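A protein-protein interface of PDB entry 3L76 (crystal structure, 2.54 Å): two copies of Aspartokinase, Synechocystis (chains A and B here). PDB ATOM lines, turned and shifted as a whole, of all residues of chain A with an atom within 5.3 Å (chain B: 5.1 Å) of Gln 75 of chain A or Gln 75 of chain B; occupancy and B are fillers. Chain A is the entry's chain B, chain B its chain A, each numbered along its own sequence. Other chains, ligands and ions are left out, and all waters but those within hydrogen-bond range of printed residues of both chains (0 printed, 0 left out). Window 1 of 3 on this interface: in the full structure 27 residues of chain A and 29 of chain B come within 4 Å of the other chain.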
ATOM      1  N   MET A  68     -22.796   4.263  27.210  1.00  0.00           N
ATOM      2  CA  MET A  68     -21.389   3.908  27.171  1.00  0.00           C
ATOM      3  C   MET A  68     -21.202   2.821  26.128  1.00  0.00           C
ATOM      4  O   MET A  68     -20.323   2.900  25.273  1.00  0.00           O
ATOM      5  CB  MET A  68     -20.940   3.396  28.533  1.00  0.00           C
ATOM      6  CG  MET A  68     -19.439   3.316  28.699  1.00  0.00           C
ATOM      7  SD  MET A  68     -19.064   2.280  30.110  1.00  0.00           S
ATOM      8  CE  MET A  68     -20.397   2.755  31.207  1.00  0.00           C
ATOM      9  N   SER A  71     -21.668   4.124  22.732  1.00  0.00           N
ATOM     10  CA  SER A  71     -20.654   5.143  22.455  1.00  0.00           C
ATOM     11  C   SER A  71     -19.372   4.598  21.825  1.00  0.00           C
ATOM     12  O   SER A  71     -18.594   5.369  21.260  1.00  0.00           O
ATOM     13  CB  SER A  71     -20.299   5.924  23.720  1.00  0.00           C
ATOM     14  OG  SER A  71     -19.003   5.577  24.176  1.00  0.00           O
ATOM     15  N   THR A  72     -19.148   3.284  21.918  1.00  0.00           N
ATOM     16  CA  THR A  72     -17.899   2.692  21.423  1.00  0.00           C
ATOM     17  C   THR A  72     -17.797   2.733  19.903  1.00  0.00           C
ATOM     18  O   THR A  72     -16.697   2.780  19.353  1.00  0.00           O
ATOM     19  CB  THR A  72     -17.685   1.241  21.918  1.00  0.00           C
ATOM     20  OG1 THR A  72     -18.599   0.355  21.266  1.00  0.00           O
ATOM     21  CG2 THR A  72     -17.868   1.151  23.422  1.00  0.00           C
ATOM     22  N   GLY A  73     -18.949   2.733  19.235  1.00  0.00           N
ATOM     23  CA  GLY A  73     -19.010   2.707  17.783  1.00  0.00           C
ATOM     24  C   GLY A  73     -18.196   3.780  17.088  1.00  0.00           C
ATOM     25  O   GLY A  73     -17.290   3.478  16.307  1.00  0.00           O
ATOM     26  N   GLU A  74     -18.526   5.039  17.355  1.00  0.00           N
ATOM     27  CA  GLU A  74     -17.830   6.155  16.723  1.00  0.00           C
ATOM     28  C   GLU A  74     -16.412   6.251  17.268  1.00  0.00           C
ATOM     29  O   GLU A  74     -15.499   6.739  16.598  1.00  0.00           O
ATOM     30  CB  GLU A  74     -18.588   7.475  16.931  1.00  0.00           C
ATOM     31  CG  GLU A  74     -19.403   7.546  18.212  1.00  0.00           C
ATOM     32  CD  GLU A  74     -20.773   6.912  18.061  1.00  0.00           C
ATOM     33  OE1 GLU A  74     -21.681   7.596  17.545  1.00  0.00           O
ATOM     34  OE2 GLU A  74     -20.943   5.736  18.459  1.00  0.00           O
ATOM     35  N   GLN A  75     -16.238   5.779  18.495  1.00  0.00           N
ATOM     36  CA  GLN A  75     -14.913   5.686  19.075  1.00  0.00           C
ATOM     37  C   GLN A  75     -14.007   4.889  18.140  1.00  0.00           C
ATOM     38  O   GLN A  75     -12.919   5.342  17.803  1.00  0.00           O
ATOM     39  CB  GLN A  75     -14.975   5.069  20.470  1.00  0.00           C
ATOM     40  CG  GLN A  75     -15.259   6.077  21.573  1.00  0.00           C
ATOM     41  CD  GLN A  75     -15.225   5.454  22.953  1.00  0.00           C
ATOM     42  OE1 GLN A  75     -14.197   4.924  23.377  1.00  0.00           O
ATOM     43  NE2 GLN A  75     -16.348   5.513  23.663  1.00  0.00           N
ATOM     44  N   VAL A  76     -14.464   3.724  17.692  1.00  0.00           N
ATOM     45  CA  VAL A  76     -13.702   2.975  16.693  1.00  0.00           C
ATOM     46  C   VAL A  76     -13.714   3.618  15.293  1.00  0.00           C
ATOM     47  O   VAL A  76     -12.663   3.712  14.665  1.00  0.00           O
ATOM     48  CB  VAL A  76     -14.081   1.464  16.634  1.00  0.00           C
ATOM     49  CG1 VAL A  76     -15.333   1.180  17.426  1.00  0.00           C
ATOM     50  CG2 VAL A  76     -14.230   0.997  15.198  1.00  0.00           C
ATOM     51  N   SER A  77     -14.873   4.076  14.812  1.00  0.00           N
ATOM     52  CA  SER A  77     -14.928   4.695  13.479  1.00  0.00           C
ATOM     53  C   SER A  77     -13.932   5.858  13.293  1.00  0.00           C
ATOM     54  O   SER A  77     -13.223   5.926  12.289  1.00  0.00           O
ATOM     55  CB  SER A  77     -16.355   5.132  13.117  1.00  0.00           C
ATOM     56  OG  SER A  77     -17.235   4.017  13.090  1.00  0.00           O
ATOM     57  N   ILE A  78     -13.862   6.767  14.259  1.00  0.00           N
ATOM     58  CA  ILE A  78     -12.908   7.871  14.155  1.00  0.00           C
ATOM     59  C   ILE A  78     -11.456   7.388  14.322  1.00  0.00           C
ATOM     60  O   ILE A  78     -10.517   7.978  13.769  1.00  0.00           O
ATOM     61  CB  ILE A  78     -13.221   9.017  15.144  1.00  0.00           C
ATOM     62  CG1 ILE A  78     -12.900   8.602  16.578  1.00  0.00           C
ATOM     63  CG2 ILE A  78     -14.684   9.467  15.005  1.00  0.00           C
ATOM     64  CD1 ILE A  78     -12.957   9.755  17.567  1.00  0.00           C
ATOM     65  N   ALA A  79     -11.263   6.307  15.068  1.00  0.00           N
ATOM     66  CA  ALA A  79      -9.925   5.726  15.171  1.00  0.00           C
ATOM     67  C   ALA A  79      -9.505   5.161  13.815  1.00  0.00           C
ATOM     68  O   ALA A  79      -8.420   5.468  13.305  1.00  0.00           O
ATOM     69  CB  ALA A  79      -9.862   4.646  16.258  1.00  0.00           C
ATOM     70  N   THR A  96     -12.331  13.245  21.422  1.00  0.00           N
ATOM     71  CA  THR A  96     -13.425  12.525  22.057  1.00  0.00           C
ATOM     72  C   THR A  96     -13.927  13.280  23.294  1.00  0.00           C
ATOM     73  O   THR A  96     -13.206  14.112  23.861  1.00  0.00           O
ATOM     74  CB  THR A  96     -12.962  11.093  22.449  1.00  0.00           C
ATOM     75  OG1 THR A  96     -13.786  10.111  21.803  1.00  0.00           O
ATOM     76  CG2 THR A  96     -13.015  10.895  23.956  1.00  0.00           C
ATOM     77  N   ALA A 134     -15.685  12.569  17.859  1.00  0.00           N
ATOM     78  CA  ALA A 134     -16.741  11.674  18.296  1.00  0.00           C
ATOM     79  C   ALA A 134     -16.897  11.755  19.808  1.00  0.00           C
ATOM     80  O   ALA A 134     -15.923  11.597  20.563  1.00  0.00           O
ATOM     81  CB  ALA A 134     -16.446  10.251  17.866  1.00  0.00           C
ATOM     82  N   ILE A 147     -17.795   9.670  27.896  1.00  0.00           N
ATOM     83  CA  ILE A 147     -18.141   9.763  26.468  1.00  0.00           C
ATOM     84  C   ILE A 147     -19.546   9.222  26.182  1.00  0.00           C
ATOM     85  O   ILE A 147     -19.849   8.064  26.477  1.00  0.00           O
ATOM     86  CB  ILE A 147     -17.138   9.002  25.549  1.00  0.00           C
ATOM     87  CG1 ILE A 147     -15.702   9.126  26.062  1.00  0.00           C
ATOM     88  CG2 ILE A 147     -17.237   9.503  24.108  1.00  0.00           C
ATOM     89  CD1 ILE A 147     -14.708   8.366  25.235  1.00  0.00           C
ATOM     90  N   MET B  68      -6.830   3.952  21.871  1.00  0.00           N
ATOM     91  CA  MET B  68      -8.248   4.291  21.802  1.00  0.00           C
ATOM     92  C   MET B  68      -9.041   3.116  21.237  1.00  0.00           C
ATOM     93  O   MET B  68      -9.963   2.601  21.877  1.00  0.00           O
ATOM     94  CB  MET B  68      -8.477   5.535  20.929  1.00  0.00           C
ATOM     95  CG  MET B  68      -9.965   5.832  20.644  1.00  0.00           C
ATOM     96  SD  MET B  68     -10.270   7.305  19.628  1.00  0.00           S
ATOM     97  CE  MET B  68      -8.906   7.174  18.463  1.00  0.00           C
ATOM     98  N   SER B  71      -9.214   0.236  23.424  1.00  0.00           N
ATOM     99  CA  SER B  71      -9.970   0.604  24.618  1.00  0.00           C
ATOM    100  C   SER B  71     -11.470   0.355  24.492  1.00  0.00           C
ATOM    101  O   SER B  71     -12.152   0.189  25.503  1.00  0.00           O
ATOM    102  CB  SER B  71      -9.745   2.078  24.958  1.00  0.00           C
ATOM    103  OG  SER B  71     -10.891   2.619  25.587  1.00  0.00           O
ATOM    104  N   THR B  72     -11.986   0.338  23.264  1.00  0.00           N
ATOM    105  CA  THR B  72     -13.435   0.250  23.070  1.00  0.00           C
ATOM    106  C   THR B  72     -14.015  -1.112  23.447  1.00  0.00           C
ATOM    107  O   THR B  72     -15.159  -1.195  23.913  1.00  0.00           O
ATOM    108  CB  THR B  72     -13.856   0.584  21.631  1.00  0.00           C
ATOM    109  OG1 THR B  72     -13.375  -0.434  20.749  1.00  0.00           O
ATOM    110  CG2 THR B  72     -13.323   1.957  21.208  1.00  0.00           C
ATOM    111  N   GLY B  73     -13.226  -2.168  23.250  1.00  0.00           N
ATOM    112  CA  GLY B  73     -13.656  -3.513  23.601  1.00  0.00           C
ATOM    113  C   GLY B  73     -13.839  -3.675  25.098  1.00  0.00           C
ATOM    114  O   GLY B  73     -14.711  -4.413  25.564  1.00  0.00           O
ATOM    115  N   GLU B  74     -13.002  -2.966  25.845  1.00  0.00           N
ATOM    116  CA  GLU B  74     -13.046  -2.962  27.296  1.00  0.00           C
ATOM    117  C   GLU B  74     -14.260  -2.183  27.770  1.00  0.00           C
ATOM    118  O   GLU B  74     -14.927  -2.568  28.735  1.00  0.00           O
ATOM    119  CB  GLU B  74     -11.775  -2.320  27.848  1.00  0.00           C
ATOM    120  CG  GLU B  74     -10.518  -2.717  27.094  1.00  0.00           C
ATOM    121  CD  GLU B  74      -9.428  -3.196  28.027  1.00  0.00           C
ATOM    122  OE1 GLU B  74      -9.059  -2.436  28.952  1.00  0.00           O
ATOM    123  OE2 GLU B  74      -8.948  -4.337  27.839  1.00  0.00           O
ATOM    124  N   GLN B  75     -14.554  -1.087  27.084  1.00  0.00           N
ATOM    125  CA  GLN B  75     -15.724  -0.296  27.440  1.00  0.00           C
ATOM    126  C   GLN B  75     -17.017  -1.071  27.274  1.00  0.00           C
ATOM    127  O   GLN B  75     -17.889  -0.965  28.136  1.00  0.00           O
ATOM    128  CB  GLN B  75     -15.795   0.998  26.646  1.00  0.00           C
ATOM    129  CG  GLN B  75     -14.827   2.049  27.094  1.00  0.00           C
ATOM    130  CD  GLN B  75     -14.746   3.177  26.100  1.00  0.00           C
ATOM    131  OE1 GLN B  75     -15.696   3.953  25.952  1.00  0.00           O
ATOM    132  NE2 GLN B  75     -13.615   3.270  25.395  1.00  0.00           N
ATOM    133  N   VAL B  76     -17.165  -1.835  26.186  1.00  0.00           N
ATOM    134  CA  VAL B  76     -18.450  -2.519  25.988  1.00  0.00           C
ATOM    135  C   VAL B  76     -18.627  -3.579  27.061  1.00  0.00           C
ATOM    136  O   VAL B  76     -19.723  -3.789  27.575  1.00  0.00           O
ATOM    137  CB  VAL B  76     -18.708  -3.102  24.542  1.00  0.00           C
ATOM    138  CG1 VAL B  76     -17.827  -2.457  23.488  1.00  0.00           C
ATOM    139  CG2 VAL B  76     -18.625  -4.632  24.511  1.00  0.00           C
ATOM    140  N   SER B  77     -17.522  -4.206  27.433  1.00  0.00           N
ATOM    141  CA  SER B  77     -17.537  -5.272  28.432  1.00  0.00           C
ATOM    142  C   SER B  77     -17.991  -4.832  29.836  1.00  0.00           C
ATOM    143  O   SER B  77     -18.804  -5.506  30.469  1.00  0.00           O
ATOM    144  CB  SER B  77     -16.157  -5.945  28.498  1.00  0.00           C
ATOM    145  OG  SER B  77     -15.783  -6.476  27.234  1.00  0.00           O
ATOM    146  N   ILE B  78     -17.466  -3.716  30.335  1.00  0.00           N
ATOM    147  CA  ILE B  78     -17.900  -3.226  31.644  1.00  0.00           C
ATOM    148  C   ILE B  78     -19.350  -2.719  31.630  1.00  0.00           C
ATOM    149  O   ILE B  78     -20.052  -2.805  32.637  1.00  0.00           O
ATOM    150  CB  ILE B  78     -16.944  -2.149  32.213  1.00  0.00           C
ATOM    151  CG1 ILE B  78     -17.111  -0.817  31.476  1.00  0.00           C
ATOM    152  CG2 ILE B  78     -15.481  -2.643  32.169  1.00  0.00           C
ATOM    153  CD1 ILE B  78     -16.339   0.331  32.123  1.00  0.00           C
ATOM    154  N   ALA B  79     -19.799  -2.195  30.492  1.00  0.00           N
ATOM    155  CA  ALA B  79     -21.196  -1.806  30.349  1.00  0.00           C
ATOM    156  C   ALA B  79     -22.068  -3.053  30.460  1.00  0.00           C
ATOM    157  O   ALA B  79     -22.986  -3.115  31.277  1.00  0.00           O
ATOM    158  CB  ALA B  79     -21.431  -1.078  29.015  1.00  0.00           C
ATOM    159  N   THR B  96     -14.660   4.865  34.075  1.00  0.00           N
ATOM    160  CA  THR B  96     -13.852   4.935  32.864  1.00  0.00           C
ATOM    161  C   THR B  96     -12.861   6.096  32.951  1.00  0.00           C
ATOM    162  O   THR B  96     -13.076   7.051  33.704  1.00  0.00           O
ATOM    163  CB  THR B  96     -14.754   5.132  31.618  1.00  0.00           C
ATOM    164  OG1 THR B  96     -14.579   4.048  30.700  1.00  0.00           O
ATOM    165  CG2 THR B  96     -14.444   6.449  30.921  1.00  0.00           C
ATOM    166  N   ALA B 134     -12.757   0.393  33.608  1.00  0.00           N
ATOM    167  CA  ALA B 134     -12.088   0.240  32.332  1.00  0.00           C
ATOM    168  C   ALA B 134     -11.582   1.591  31.844  1.00  0.00           C
ATOM    169  O   ALA B 134     -12.334   2.573  31.763  1.00  0.00           O
ATOM    170  CB  ALA B 134     -13.022  -0.381  31.313  1.00  0.00           C
ATOM    171  N   ILE B 147      -9.912   8.206  26.958  1.00  0.00           N
ATOM    172  CA  ILE B 147      -9.882   6.812  27.413  1.00  0.00           C
ATOM    173  C   ILE B 147      -8.901   5.965  26.587  1.00  0.00           C
ATOM    174  O   ILE B 147      -9.018   5.860  25.363  1.00  0.00           O
ATOM    175  CB  ILE B 147     -11.277   6.128  27.378  1.00  0.00           C
ATOM    176  CG1 ILE B 147     -12.385   7.089  27.809  1.00  0.00           C
ATOM    177  CG2 ILE B 147     -11.281   4.893  28.265  1.00  0.00           C
ATOM    178  CD1 ILE B 147     -13.764   6.492  27.727  1.00  0.00           C
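OG of Ser 71 of chain B lies within hydrogen-bond range of NE2 of Gln 75 of chain B, 2.8 Å away. The backbone carbonyl oxygen (O) of Met 68 of chain A is in hydrogen-bond range of the side-chain hydroxyl (OG) of Ser 71 of chain A. The side-chain amide nitrogen (NE2) of Gln 75 of chain A sits at hydrogen-bond distance from the side-chain hydroxyl (OG) of Ser 71 of chain A. O of Ile 147 of chain A is in hydrogen-bond range of OG of Ser 71 of chain A.
Gln 75 of chain A touches just these residues of chain B: Met 68, Thr 72 and Gln 75. Printed residues of chain A within 4 Å of Gln 75 of chain B: Met 68, Thr 72 and Gln 75. Of the printed residues of chain B, Thr 72 of chain A touches Thr 72, Gln 75 and Val 76. Of the printed residues of chain A, Ile 78 of chain B touches Met 68 (3.9 Å). Of the printed residues of chain A, Val 76 of chain B touches Thr 72 (3.6 Å). Ala 134 of chain A touches none of the printed residues of chain B. Gly 73 of chain B touches none of the printed residues of chain A. The nearest residue of chain B that does not touch Gln 75 of chain A is Ser 71 of chain B (4.6 Å). The nearest residue of chain A that does not touch Gln 75 of chain B is Ser 71 of chain A (4.1 Å). The nearest printed residue of chain B that does not touch Thr 72 of chain A is Gly 73 of chain B (5.7 Å).
Met 68 of chain A touches Gln 75 of chain B (SD to O, 3.98 Å). Met 68 of chain A touches Ile 78 of chain B (SD to CG1, 3.9 Å). Thr 72 of chain B touches Thr 72 of chain A. Gln 75 of chain B touches Thr 72 of chain A. CG2 of Thr 72 of chain A touches CG1 of Val 76 of chain B, 3.6 Å away. Gln 75 of chain A touches Thr 72 of chain B. Ala 79 of chain A touches Met 68 of chain B. CD1 of Ile 147 of chain A touches CD1 of Ile 147 of chain B, at 3.3 Å.
Of the 13 printed residues of chain B, 6 touch a printed residue of chain A. Printed residues of chain B that touch a printed residue of chain A: Met 68, Thr 72, Gln 75, Val 76, Ile 78 and Ile 147. Hydrophobic or aromatic side chains of chain B within 4 Å of the printed part of chain A: Met 68, Val 76, Ile 78 and Ile 147. Of the 13 printed residues of chain A, 5 touch a printed residue of chain B. Hydrophobic or aromatic side chains of chain A within 4 Å of the printed part of chain B: Met 68, Ala 79 and Ile 147. Along chain A the printed residues that touch a printed residue of chain B span positions 68 to 147. Among the printed residues, 10 pairs touch across the chains. Among the printed residues, no Asp or Glu carboxylate lies within 4 Å of a Lys or Arg side-chain nitrogen of the other chain.
NE2 of Gln 75 of chain B lies within hydrogen-bond range of OE1 of Gln 75 of chain A, 2.7 Å away. O of Gln 75 of chain A lies close to SD of Met 68 of chain B (3.8 Å).
Thr 72 of chain A touches its own counterpart, Thr 72 of chain B. Thr 72 of chain A touches Gln 75 of chain B, and with the chains exchanged Gln 75 of chain A touches Thr 72 of chain B. Thr 72 of chain A touches Val 76 of chain B, but with the chains exchanged Val 76 of chain A does not touch Thr 72 of chain B (4.1 Å). Gln 75 of chain A touches its own counterpart, Gln 75 of chain B. Positions printed for both chains: 68, 71, 72, 73, 74, 75, 76, 77, 78, 79, 96, 134 and 147. Of the 10 pairs that touch across the chains among the printed residues, 7 have their exchanged pair printed and touching as well.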
